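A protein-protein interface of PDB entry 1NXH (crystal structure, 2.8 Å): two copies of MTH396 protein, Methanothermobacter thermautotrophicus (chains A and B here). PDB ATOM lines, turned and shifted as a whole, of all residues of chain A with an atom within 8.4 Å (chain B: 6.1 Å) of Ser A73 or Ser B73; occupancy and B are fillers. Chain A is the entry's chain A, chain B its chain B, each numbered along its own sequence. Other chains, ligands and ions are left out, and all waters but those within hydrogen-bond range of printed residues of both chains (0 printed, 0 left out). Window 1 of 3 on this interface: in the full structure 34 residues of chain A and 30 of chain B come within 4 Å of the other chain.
The side-chain sulfur (SG) of Cys B78 is disulfide-bonded to the side-chain sulfur (SG) of Cys A66 (2.0 Å).
The side-chain amino group of Lys A70 lies within hydrogen-bond range of the side-chain amide oxygen of Gln B76 (3.0 Å).
SG of Cys A78 is disulfide-bonded to SG of Cys B66, 2.0 Å away.
SG of Cys B66 lies close to NE1 of Trp A79 (3.7 Å).
SG of Cys B78 lies close to OE2 of Glu A69 (3.6 Å).
The side-chain sulfur (SG) of Cys A78 lies close to the side-chain carboxylate (OE2) of Glu B69.
NE2 of Gln A76 is in hydrogen-bond range of O of Asp A74, 3.4 Å away.
OD1 of Asp A74 lies within hydrogen-bond range of OH of Tyr A109 (2.5 Å).
The backbone NH of Leu B77 is in hydrogen-bond range of the backbone carbonyl oxygen of His B72 (2.9 Å).
O of Asp B74 sits close to OE1 of Gln B76, 3.4 Å away.
Arg A30 touches Gln B76 (CB to CD, 3.3 Å).
Glu A31 touches Gln B76 (OE1 to CB, 3.3 Å).
His B72 touches Glu A69 (CD2 to OE2, 3.6 Å).
Lys A70 touches Ser B73 (CA to OG, 3.3 Å).
Lys B70 touches Ser A73.
OG of Ser B73 touches CB of Ser A73, at 3.7 Å.
Asp A74 touches Asp B74 (OD2 to OD1, 3.9 Å).
Gln A76 touches Lys B70.
Printed residues of chain B within 4 Å of Arg A30: Gln B76 (3.3 Å).
Printed residues of chain B within 4 Å of Cys A66: Cys B78.
Ser A73 touches just these residues of chain B: Lys B70 (3.5 Å) and Ser B73 (3.7 Å).
Ser B73 touches just these residues of chain A: Lys A70 (3.3 Å) and Ser A73 (3.7 Å).
Printed residues of chain A within 4 Å of Asp B74: Asp A74 (3.9 Å).
Leu B75 touches none of the printed residues of chain A.
The nearest residue of chain B that does not touch Ser A73 is Glu B69 (4.5 Å).
The nearest residue of chain A that does not touch Ser B73 is Glu A69 (4.1 Å).
Among the printed residues, 14 pairs touch across the chains.
Cys A66 touches Cys B78, and with the chains exchanged Cys A78 touches Cys B66.
Glu A69 touches Cys B78, and with the chains exchanged Cys A78 touches Glu B69.
Lys A70 touches Gln B76, and with the chains exchanged Gln A76 touches Lys B70.
Asp B74 touches its own counterpart, Asp A74.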
ATOM      1  N   LEU A  28     -25.600 -21.696   2.463  1.00  0.00           N
ATOM      2  CA  LEU A  28     -24.546 -22.609   2.882  1.00  0.00           C
ATOM      3  C   LEU A  28     -24.494 -23.813   1.955  1.00  0.00           C
ATOM      4  O   LEU A  28     -24.498 -24.961   2.406  1.00  0.00           O
ATOM      5  CB  LEU A  28     -24.766 -23.059   4.329  1.00  0.00           C
ATOM      6  CG  LEU A  28     -24.293 -22.021   5.362  1.00  0.00           C
ATOM      7  CD1 LEU A  28     -24.926 -22.261   6.726  1.00  0.00           C
ATOM      8  CD2 LEU A  28     -22.776 -22.079   5.447  1.00  0.00           C
ATOM      9  N   ARG A  30     -22.070 -23.891  -0.087  1.00  0.00           N
ATOM     10  CA  ARG A  30     -20.635 -23.909  -0.292  1.00  0.00           C
ATOM     11  C   ARG A  30     -19.956 -25.231   0.065  1.00  0.00           C
ATOM     12  O   ARG A  30     -18.733 -25.338  -0.048  1.00  0.00           O
ATOM     13  CB  ARG A  30     -19.985 -22.765   0.497  1.00  0.00           C
ATOM     14  CG  ARG A  30     -19.919 -21.442  -0.248  1.00  0.00           C
ATOM     15  CD  ARG A  30     -18.853 -21.462  -1.346  1.00  0.00           C
ATOM     16  NE  ARG A  30     -18.941 -22.658  -2.191  1.00  0.00           N
ATOM     17  CZ  ARG A  30     -18.344 -22.810  -3.376  1.00  0.00           C
ATOM     18  NH1 ARG A  30     -17.597 -21.838  -3.891  1.00  0.00           N
ATOM     19  NH2 ARG A  30     -18.495 -23.947  -4.053  1.00  0.00           N
ATOM     20  N   GLU A  31     -20.722 -26.232   0.501  1.00  0.00           N
ATOM     21  CA  GLU A  31     -20.135 -27.535   0.844  1.00  0.00           C
ATOM     22  C   GLU A  31     -20.599 -28.562  -0.148  1.00  0.00           C
ATOM     23  O   GLU A  31     -20.918 -29.685   0.240  1.00  0.00           O
ATOM     24  CB  GLU A  31     -20.591 -28.035   2.219  1.00  0.00           C
ATOM     25  CG  GLU A  31     -20.036 -27.312   3.421  1.00  0.00           C
ATOM     26  CD  GLU A  31     -20.856 -26.099   3.811  1.00  0.00           C
ATOM     27  OE1 GLU A  31     -20.526 -25.494   4.848  1.00  0.00           O
ATOM     28  OE2 GLU A  31     -21.821 -25.747   3.091  1.00  0.00           O
ATOM     29  N   CYS A  66     -17.863 -12.284   8.754  1.00  0.00           N
ATOM     30  CA  CYS A  66     -17.541 -13.510   8.064  1.00  0.00           C
ATOM     31  C   CYS A  66     -17.186 -13.317   6.602  1.00  0.00           C
ATOM     32  O   CYS A  66     -16.438 -14.118   6.013  1.00  0.00           O
ATOM     33  CB  CYS A  66     -18.692 -14.494   8.208  1.00  0.00           C
ATOM     34  SG  CYS A  66     -18.745 -15.312   9.841  1.00  0.00           S
ATOM     35  N   ILE A  67     -17.709 -12.248   6.015  1.00  0.00           N
ATOM     36  CA  ILE A  67     -17.429 -11.971   4.615  1.00  0.00           C
ATOM     37  C   ILE A  67     -16.043 -11.374   4.464  1.00  0.00           C
ATOM     38  O   ILE A  67     -15.313 -11.711   3.532  1.00  0.00           O
ATOM     39  CB  ILE A  67     -18.456 -11.000   4.010  1.00  0.00           C
ATOM     40  CG1 ILE A  67     -19.863 -11.616   4.083  1.00  0.00           C
ATOM     41  CG2 ILE A  67     -18.051 -10.680   2.568  1.00  0.00           C
ATOM     42  CD1 ILE A  67     -20.978 -10.690   3.675  1.00  0.00           C
ATOM     43  N   ARG A  68     -15.687 -10.482   5.381  1.00  0.00           N
ATOM     44  CA  ARG A  68     -14.374  -9.864   5.336  1.00  0.00           C
ATOM     45  C   ARG A  68     -13.370 -10.981   5.384  1.00  0.00           C
ATOM     46  O   ARG A  68     -12.447 -11.026   4.575  1.00  0.00           O
ATOM     47  CB  ARG A  68     -14.154  -8.940   6.524  1.00  0.00           C
ATOM     48  CG  ARG A  68     -15.246  -7.928   6.676  1.00  0.00           C
ATOM     49  CD  ARG A  68     -14.790  -6.784   7.507  1.00  0.00           C
ATOM     50  NE  ARG A  68     -13.552  -6.215   6.986  1.00  0.00           N
ATOM     51  CZ  ARG A  68     -13.326  -4.905   6.947  1.00  0.00           C
ATOM     52  NH1 ARG A  68     -14.262  -4.067   7.391  1.00  0.00           N
ATOM     53  NH2 ARG A  68     -12.179  -4.425   6.476  1.00  0.00           N
ATOM     54  N   GLU A  69     -13.560 -11.897   6.329  1.00  0.00           N
ATOM     55  CA  GLU A  69     -12.659 -13.030   6.462  1.00  0.00           C
ATOM     56  C   GLU A  69     -12.476 -13.728   5.119  1.00  0.00           C
ATOM     57  O   GLU A  69     -11.339 -13.915   4.654  1.00  0.00           O
ATOM     58  CB  GLU A  69     -13.198 -14.037   7.468  1.00  0.00           C
ATOM     59  CG  GLU A  69     -13.015 -13.651   8.918  1.00  0.00           C
ATOM     60  CD  GLU A  69     -13.262 -14.825   9.846  1.00  0.00           C
ATOM     61  OE1 GLU A  69     -13.401 -14.594  11.070  1.00  0.00           O
ATOM     62  OE2 GLU A  69     -13.310 -15.978   9.352  1.00  0.00           O
ATOM     63  N   LYS A  70     -13.600 -14.107   4.502  1.00  0.00           N
ATOM     64  CA  LYS A  70     -13.586 -14.788   3.208  1.00  0.00           C
ATOM     65  C   LYS A  70     -12.782 -13.939   2.214  1.00  0.00           C
ATOM     66  O   LYS A  70     -11.880 -14.437   1.539  1.00  0.00           O
ATOM     67  CB  LYS A  70     -15.032 -15.006   2.715  1.00  0.00           C
ATOM     68  CG  LYS A  70     -15.228 -16.267   1.841  1.00  0.00           C
ATOM     69  CD  LYS A  70     -16.718 -16.624   1.621  1.00  0.00           C
ATOM     70  CE  LYS A  70     -16.964 -17.659   0.468  1.00  0.00           C
ATOM     71  NZ  LYS A  70     -16.539 -19.079   0.735  1.00  0.00           N
ATOM     72  N   LEU A  71     -13.092 -12.649   2.154  1.00  0.00           N
ATOM     73  CA  LEU A  71     -12.393 -11.745   1.244  1.00  0.00           C
ATOM     74  C   LEU A  71     -10.895 -11.744   1.489  1.00  0.00           C
ATOM     75  O   LEU A  71     -10.100 -11.964   0.579  1.00  0.00           O
ATOM     76  CB  LEU A  71     -12.932 -10.319   1.390  1.00  0.00           C
ATOM     77  CG  LEU A  71     -14.396 -10.209   0.973  1.00  0.00           C
ATOM     78  CD1 LEU A  71     -14.948  -8.836   1.288  1.00  0.00           C
ATOM     79  CD2 LEU A  71     -14.500 -10.533  -0.517  1.00  0.00           C
ATOM     80  N   HIS A  72     -10.521 -11.490   2.732  1.00  0.00           N
ATOM     81  CA  HIS A  72      -9.122 -11.446   3.098  1.00  0.00           C
ATOM     82  C   HIS A  72      -8.415 -12.661   2.531  1.00  0.00           C
ATOM     83  O   HIS A  72      -7.345 -12.549   1.920  1.00  0.00           O
ATOM     84  CB  HIS A  72      -8.975 -11.439   4.617  1.00  0.00           C
ATOM     85  CG  HIS A  72      -7.618 -11.019   5.075  1.00  0.00           C
ATOM     86  ND1 HIS A  72      -7.192  -9.708   5.026  1.00  0.00           N
ATOM     87  CD2 HIS A  72      -6.565 -11.742   5.525  1.00  0.00           C
ATOM     88  CE1 HIS A  72      -5.933  -9.640   5.429  1.00  0.00           C
ATOM     89  NE2 HIS A  72      -5.528 -10.860   5.735  1.00  0.00           N
ATOM     90  N   SER A  73      -9.037 -13.818   2.741  1.00  0.00           N
ATOM     91  CA  SER A  73      -8.492 -15.085   2.281  1.00  0.00           C
ATOM     92  C   SER A  73      -8.445 -15.171   0.773  1.00  0.00           C
ATOM     93  O   SER A  73      -7.375 -15.269   0.181  1.00  0.00           O
ATOM     94  CB  SER A  73      -9.313 -16.256   2.792  1.00  0.00           C
ATOM     95  OG  SER A  73      -8.866 -17.442   2.159  1.00  0.00           O
ATOM     96  N   ASP A  74      -9.613 -15.136   0.152  1.00  0.00           N
ATOM     97  CA  ASP A  74      -9.700 -15.219  -1.292  1.00  0.00           C
ATOM     98  C   ASP A  74      -8.796 -14.240  -2.027  1.00  0.00           C
ATOM     99  O   ASP A  74      -8.318 -14.545  -3.126  1.00  0.00           O
ATOM    100  CB  ASP A  74     -11.142 -15.004  -1.722  1.00  0.00           C
ATOM    101  CG  ASP A  74     -12.040 -16.093  -1.233  1.00  0.00           C
ATOM    102  OD1 ASP A  74     -13.259 -15.987  -1.453  1.00  0.00           O
ATOM    103  OD2 ASP A  74     -11.520 -17.064  -0.632  1.00  0.00           O
ATOM    104  N   LEU A  75      -8.568 -13.071  -1.428  1.00  0.00           N
ATOM    105  CA  LEU A  75      -7.722 -12.054  -2.039  1.00  0.00           C
ATOM    106  C   LEU A  75      -6.260 -12.173  -1.633  1.00  0.00           C
ATOM    107  O   LEU A  75      -5.517 -11.200  -1.664  1.00  0.00           O
ATOM    108  CB  LEU A  75      -8.232 -10.661  -1.698  1.00  0.00           C
ATOM    109  CG  LEU A  75      -9.609 -10.310  -2.268  1.00  0.00           C
ATOM    110  CD1 LEU A  75      -9.903  -8.834  -1.995  1.00  0.00           C
ATOM    111  CD2 LEU A  75      -9.633 -10.572  -3.766  1.00  0.00           C
ATOM    112  N   GLN A  76      -5.858 -13.373  -1.246  1.00  0.00           N
ATOM    113  CA  GLN A  76      -4.479 -13.638  -0.871  1.00  0.00           C
ATOM    114  C   GLN A  76      -3.865 -12.523  -0.026  1.00  0.00           C
ATOM    115  O   GLN A  76      -2.690 -12.144  -0.212  1.00  0.00           O
ATOM    116  CB  GLN A  76      -3.648 -13.852  -2.137  1.00  0.00           C
ATOM    117  CG  GLN A  76      -4.297 -14.786  -3.192  1.00  0.00           C
ATOM    118  CD  GLN A  76      -4.590 -16.213  -2.686  1.00  0.00           C
ATOM    119  OE1 GLN A  76      -3.756 -16.837  -2.017  1.00  0.00           O
ATOM    120  NE2 GLN A  76      -5.776 -16.735  -3.027  1.00  0.00           N
ATOM    121  N   LEU A  77      -4.653 -12.010   0.917  1.00  0.00           N
ATOM    122  CA  LEU A  77      -4.181 -10.943   1.768  1.00  0.00           C
ATOM    123  C   LEU A  77      -3.313 -11.395   2.912  1.00  0.00           C
ATOM    124  O   LEU A  77      -2.593 -10.589   3.501  1.00  0.00           O
ATOM    125  CB  LEU A  77      -5.358 -10.145   2.278  1.00  0.00           C
ATOM    126  CG  LEU A  77      -6.000  -9.396   1.122  1.00  0.00           C
ATOM    127  CD1 LEU A  77      -7.146  -8.603   1.668  1.00  0.00           C
ATOM    128  CD2 LEU A  77      -4.986  -8.481   0.453  1.00  0.00           C
ATOM    129  N   CYS A  78      -3.375 -12.679   3.237  1.00  0.00           N
ATOM    130  CA  CYS A  78      -2.525 -13.199   4.304  1.00  0.00           C
ATOM    131  C   CYS A  78      -1.103 -12.886   3.859  1.00  0.00           C
ATOM    132  O   CYS A  78      -0.262 -12.470   4.654  1.00  0.00           O
ATOM    133  CB  CYS A  78      -2.691 -14.721   4.441  1.00  0.00           C
ATOM    134  SG  CYS A  78      -1.782 -15.535   5.810  1.00  0.00           S
ATOM    135  N   TRP A  79      -0.864 -13.073   2.562  1.00  0.00           N
ATOM    136  CA  TRP A  79       0.444 -12.860   1.965  1.00  0.00           C
ATOM    137  C   TRP A  79       0.706 -11.422   1.611  1.00  0.00           C
ATOM    138  O   TRP A  79       1.674 -10.812   2.078  1.00  0.00           O
ATOM    139  CB  TRP A  79       0.585 -13.701   0.701  1.00  0.00           C
ATOM    140  CG  TRP A  79       0.626 -15.147   0.972  1.00  0.00           C
ATOM    141  CD1 TRP A  79      -0.415 -16.026   0.912  1.00  0.00           C
ATOM    142  CD2 TRP A  79       1.763 -15.892   1.404  1.00  0.00           C
ATOM    143  NE1 TRP A  79       0.006 -17.287   1.285  1.00  0.00           N
ATOM    144  CE2 TRP A  79       1.341 -17.229   1.593  1.00  0.00           C
ATOM    145  CE3 TRP A  79       3.102 -15.560   1.652  1.00  0.00           C
ATOM    146  CZ2 TRP A  79       2.208 -18.234   2.018  1.00  0.00           C
ATOM    147  CZ3 TRP A  79       3.967 -16.556   2.073  1.00  0.00           C
ATOM    148  CH2 TRP A  79       3.516 -17.881   2.252  1.00  0.00           C
ATOM    149  N   LEU A  80      -0.159 -10.884   0.768  1.00  0.00           N
ATOM    150  CA  LEU A  80       0.010  -9.519   0.337  1.00  0.00           C
ATOM    151  C   LEU A  80       0.164  -8.526   1.469  1.00  0.00           C
ATOM    152  O   LEU A  80       0.794  -7.494   1.304  1.00  0.00           O
ATOM    153  CB  LEU A  80      -1.156  -9.119  -0.555  1.00  0.00           C
ATOM    154  CG  LEU A  80      -0.888  -9.389  -2.029  1.00  0.00           C
ATOM    155  CD1 LEU A  80       0.051 -10.558  -2.184  1.00  0.00           C
ATOM    156  CD2 LEU A  80      -2.199  -9.655  -2.729  1.00  0.00           C
ATOM    157  N   LYS A  96     -11.601  -4.227   1.625  1.00  0.00           N
ATOM    158  CA  LYS A  96     -12.499  -5.214   2.199  1.00  0.00           C
ATOM    159  C   LYS A  96     -13.832  -4.552   2.521  1.00  0.00           C
ATOM    160  O   LYS A  96     -14.891  -5.170   2.383  1.00  0.00           O
ATOM    161  CB  LYS A  96     -11.860  -5.833   3.445  1.00  0.00           C
ATOM    162  CG  LYS A  96     -10.719  -6.799   3.108  1.00  0.00           C
ATOM    163  CD  LYS A  96      -9.619  -6.815   4.170  1.00  0.00           C
ATOM    164  CE  LYS A  96     -10.086  -7.466   5.477  1.00  0.00           C
ATOM    165  NZ  LYS A  96      -9.054  -7.353   6.557  1.00  0.00           N
ATOM    166  N   TYR A 109     -21.452 -12.871  -4.066  1.00  0.00           N
ATOM    167  CA  TYR A 109     -20.053 -12.990  -3.644  1.00  0.00           C
ATOM    168  C   TYR A 109     -19.162 -13.213  -4.847  1.00  0.00           C
ATOM    169  O   TYR A 109     -18.268 -12.421  -5.132  1.00  0.00           O
ATOM    170  CB  TYR A 109     -19.836 -14.163  -2.676  1.00  0.00           C
ATOM    171  CG  TYR A 109     -18.422 -14.179  -2.123  1.00  0.00           C
ATOM    172  CD1 TYR A 109     -17.955 -13.104  -1.374  1.00  0.00           C
ATOM    173  CD2 TYR A 109     -17.527 -15.217  -2.415  1.00  0.00           C
ATOM    174  CE1 TYR A 109     -16.643 -13.043  -0.937  1.00  0.00           C
ATOM    175  CE2 TYR A 109     -16.195 -15.163  -1.974  1.00  0.00           C
ATOM    176  CZ  TYR A 109     -15.763 -14.062  -1.238  1.00  0.00           C
ATOM    177  OH  TYR A 109     -14.449 -13.909  -0.836  1.00  0.00           O
ATOM    178  N   LEU A 113     -16.301 -10.760  -5.596  1.00  0.00           N
ATOM    179  CA  LEU A 113     -14.891 -11.079  -5.414  1.00  0.00           C
ATOM    180  C   LEU A 113     -14.100 -10.672  -6.660  1.00  0.00           C
ATOM    181  O   LEU A 113     -12.980 -10.160  -6.562  1.00  0.00           O
ATOM    182  CB  LEU A 113     -14.722 -12.583  -5.163  1.00  0.00           C
ATOM    183  CG  LEU A 113     -13.498 -13.025  -4.355  1.00  0.00           C
ATOM    184  CD1 LEU A 113     -13.384 -14.516  -4.403  1.00  0.00           C
ATOM    185  CD2 LEU A 113     -12.223 -12.411  -4.912  1.00  0.00           C
ATOM    186  N   ARG A 117     -10.884  -8.364  -6.965  1.00  0.00           N
ATOM    187  CA  ARG A 117      -9.668  -8.836  -7.590  1.00  0.00           C
ATOM    188  C   ARG A 117      -9.198  -7.653  -8.435  1.00  0.00           C
ATOM    189  O   ARG A 117      -8.031  -7.248  -8.383  1.00  0.00           O
ATOM    190  CB  ARG A 117      -9.990 -10.028  -8.478  1.00  0.00           C
ATOM    191  CG  ARG A 117      -8.792 -10.822  -8.903  1.00  0.00           C
ATOM    192  CD  ARG A 117      -8.712 -12.077  -8.098  1.00  0.00           C
ATOM    193  NE  ARG A 117      -9.956 -12.828  -8.221  1.00  0.00           N
ATOM    194  CZ  ARG A 117     -10.210 -13.989  -7.614  1.00  0.00           C
ATOM    195  NH1 ARG A 117      -9.301 -14.560  -6.819  1.00  0.00           N
ATOM    196  NH2 ARG A 117     -11.389 -14.583  -7.804  1.00  0.00           N
ATOM    197  N   CYS B  66      -1.169 -19.283   6.787  1.00  0.00           N
ATOM    198  CA  CYS B  66      -1.945 -18.785   5.663  1.00  0.00           C
ATOM    199  C   CYS B  66      -2.859 -19.821   5.061  1.00  0.00           C
ATOM    200  O   CYS B  66      -3.914 -19.500   4.527  1.00  0.00           O
ATOM    201  CB  CYS B  66      -1.033 -18.247   4.573  1.00  0.00           C
ATOM    202  SG  CYS B  66      -0.294 -16.630   4.937  1.00  0.00           S
ATOM    203  N   ARG B  68      -4.139 -22.529   6.846  1.00  0.00           N
ATOM    204  CA  ARG B  68      -5.209 -22.817   7.775  1.00  0.00           C
ATOM    205  C   ARG B  68      -6.270 -21.767   7.529  1.00  0.00           C
ATOM    206  O   ARG B  68      -7.453 -22.098   7.374  1.00  0.00           O
ATOM    207  CB  ARG B  68      -4.730 -22.739   9.216  1.00  0.00           C
ATOM    208  CG  ARG B  68      -3.947 -23.955   9.639  1.00  0.00           C
ATOM    209  CD  ARG B  68      -3.431 -23.876  11.099  1.00  0.00           C
ATOM    210  NE  ARG B  68      -4.173 -24.716  12.059  1.00  0.00           N
ATOM    211  CZ  ARG B  68      -5.238 -24.319  12.758  1.00  0.00           C
ATOM    212  NH1 ARG B  68      -5.715 -23.083  12.631  1.00  0.00           N
ATOM    213  NH2 ARG B  68      -5.837 -25.164  13.585  1.00  0.00           N
ATOM    214  N   GLU B  69      -5.843 -20.505   7.454  1.00  0.00           N
ATOM    215  CA  GLU B  69      -6.786 -19.413   7.248  1.00  0.00           C
ATOM    216  C   GLU B  69      -7.660 -19.653   6.036  1.00  0.00           C
ATOM    217  O   GLU B  69      -8.890 -19.506   6.105  1.00  0.00           O
ATOM    218  CB  GLU B  69      -6.044 -18.088   7.135  1.00  0.00           C
ATOM    219  CG  GLU B  69      -5.436 -17.682   8.466  1.00  0.00           C
ATOM    220  CD  GLU B  69      -4.887 -16.257   8.495  1.00  0.00           C
ATOM    221  OE1 GLU B  69      -4.455 -15.821   9.594  1.00  0.00           O
ATOM    222  OE2 GLU B  69      -4.880 -15.574   7.436  1.00  0.00           O
ATOM    223  N   LYS B  70      -7.017 -20.037   4.935  1.00  0.00           N
ATOM    224  CA  LYS B  70      -7.719 -20.328   3.693  1.00  0.00           C
ATOM    225  C   LYS B  70      -8.706 -21.472   3.941  1.00  0.00           C
ATOM    226  O   LYS B  70      -9.866 -21.417   3.526  1.00  0.00           O
ATOM    227  CB  LYS B  70      -6.714 -20.714   2.614  1.00  0.00           C
ATOM    228  CG  LYS B  70      -7.255 -20.586   1.215  1.00  0.00           C
ATOM    229  CD  LYS B  70      -6.310 -19.777   0.357  1.00  0.00           C
ATOM    230  CE  LYS B  70      -6.698 -19.816  -1.117  1.00  0.00           C
ATOM    231  NZ  LYS B  70      -8.008 -19.163  -1.368  1.00  0.00           N
ATOM    232  N   LEU B  71      -8.246 -22.503   4.634  1.00  0.00           N
ATOM    233  CA  LEU B  71      -9.104 -23.633   4.946  1.00  0.00           C
ATOM    234  C   LEU B  71     -10.303 -23.182   5.765  1.00  0.00           C
ATOM    235  O   LEU B  71     -11.449 -23.398   5.367  1.00  0.00           O
ATOM    236  CB  LEU B  71      -8.326 -24.696   5.718  1.00  0.00           C
ATOM    237  CG  LEU B  71      -7.349 -25.510   4.869  1.00  0.00           C
ATOM    238  CD1 LEU B  71      -6.443 -26.367   5.748  1.00  0.00           C
ATOM    239  CD2 LEU B  71      -8.162 -26.359   3.899  1.00  0.00           C
ATOM    240  N   HIS B  72     -10.042 -22.558   6.907  1.00  0.00           N
ATOM    241  CA  HIS B  72     -11.114 -22.083   7.775  1.00  0.00           C
ATOM    242  C   HIS B  72     -12.210 -21.460   6.912  1.00  0.00           C
ATOM    243  O   HIS B  72     -13.407 -21.785   7.020  1.00  0.00           O
ATOM    244  CB  HIS B  72     -10.563 -21.024   8.745  1.00  0.00           C
ATOM    245  CG  HIS B  72     -11.547 -20.578   9.784  1.00  0.00           C
ATOM    246  ND1 HIS B  72     -11.997 -21.408  10.791  1.00  0.00           N
ATOM    247  CD2 HIS B  72     -12.190 -19.399   9.955  1.00  0.00           C
ATOM    248  CE1 HIS B  72     -12.874 -20.758  11.536  1.00  0.00           C
ATOM    249  NE2 HIS B  72     -13.010 -19.538  11.051  1.00  0.00           N
ATOM    250  N   SER B  73     -11.759 -20.564   6.046  1.00  0.00           N
ATOM    251  CA  SER B  73     -12.608 -19.831   5.147  1.00  0.00           C
ATOM    252  C   SER B  73     -13.343 -20.770   4.231  1.00  0.00           C
ATOM    253  O   SER B  73     -14.542 -20.991   4.385  1.00  0.00           O
ATOM    254  CB  SER B  73     -11.748 -18.887   4.331  1.00  0.00           C
ATOM    255  OG  SER B  73     -12.517 -17.812   3.867  1.00  0.00           O
ATOM    256  N   ASP B  74     -12.615 -21.333   3.277  1.00  0.00           N
ATOM    257  CA  ASP B  74     -13.207 -22.251   2.307  1.00  0.00           C
ATOM    258  C   ASP B  74     -14.144 -23.309   2.899  1.00  0.00           C
ATOM    259  O   ASP B  74     -15.110 -23.737   2.250  1.00  0.00           O
ATOM    260  CB  ASP B  74     -12.097 -22.922   1.491  1.00  0.00           C
ATOM    261  CG  ASP B  74     -11.310 -21.914   0.638  1.00  0.00           C
ATOM    262  OD1 ASP B  74     -11.816 -20.772   0.459  1.00  0.00           O
ATOM    263  OD2 ASP B  74     -10.207 -22.259   0.139  1.00  0.00           O
ATOM    264  N   LEU B  75     -13.868 -23.720   4.132  1.00  0.00           N
ATOM    265  CA  LEU B  75     -14.694 -24.727   4.789  1.00  0.00           C
ATOM    266  C   LEU B  75     -15.870 -24.136   5.560  1.00  0.00           C
ATOM    267  O   LEU B  75     -16.438 -24.792   6.452  1.00  0.00           O
ATOM    268  CB  LEU B  75     -13.848 -25.587   5.728  1.00  0.00           C
ATOM    269  CG  LEU B  75     -12.811 -26.496   5.061  1.00  0.00           C
ATOM    270  CD1 LEU B  75     -12.050 -27.230   6.159  1.00  0.00           C
ATOM    271  CD2 LEU B  75     -13.486 -27.479   4.107  1.00  0.00           C
ATOM    272  N   GLN B  76     -16.238 -22.904   5.198  1.00  0.00           N
ATOM    273  CA  GLN B  76     -17.368 -22.206   5.817  1.00  0.00           C
ATOM    274  C   GLN B  76     -17.325 -22.325   7.329  1.00  0.00           C
ATOM    275  O   GLN B  76     -18.376 -22.368   7.985  1.00  0.00           O
ATOM    276  CB  GLN B  76     -18.695 -22.798   5.319  1.00  0.00           C
ATOM    277  CG  GLN B  76     -18.861 -22.833   3.817  1.00  0.00           C
ATOM    278  CD  GLN B  76     -18.523 -21.507   3.178  1.00  0.00           C
ATOM    279  OE1 GLN B  76     -17.598 -21.417   2.370  1.00  0.00           O
ATOM    280  NE2 GLN B  76     -19.260 -20.463   3.544  1.00  0.00           N
ATOM    281  N   LEU B  77     -16.121 -22.364   7.888  1.00  0.00           N
ATOM    282  CA  LEU B  77     -16.011 -22.527   9.326  1.00  0.00           C
ATOM    283  C   LEU B  77     -16.356 -21.299  10.161  1.00  0.00           C
ATOM    284  O   LEU B  77     -16.455 -21.390  11.392  1.00  0.00           O
ATOM    285  CB  LEU B  77     -14.622 -23.055   9.685  1.00  0.00           C
ATOM    286  CG  LEU B  77     -14.302 -24.430   9.078  1.00  0.00           C
ATOM    287  CD1 LEU B  77     -13.026 -24.944   9.701  1.00  0.00           C
ATOM    288  CD2 LEU B  77     -15.442 -25.413   9.324  1.00  0.00           C
ATOM    289  N   CYS B  78     -16.550 -20.157   9.498  1.00  0.00           N
ATOM    290  CA  CYS B  78     -16.914 -18.929  10.209  1.00  0.00           C
ATOM    291  C   CYS B  78     -18.331 -19.127  10.723  1.00  0.00           C
ATOM    292  O   CYS B  78     -18.696 -18.645  11.791  1.00  0.00           O
ATOM    293  CB  CYS B  78     -16.882 -17.723   9.269  1.00  0.00           C
ATOM    294  SG  CYS B  78     -16.868 -16.087  10.094  1.00  0.00           S
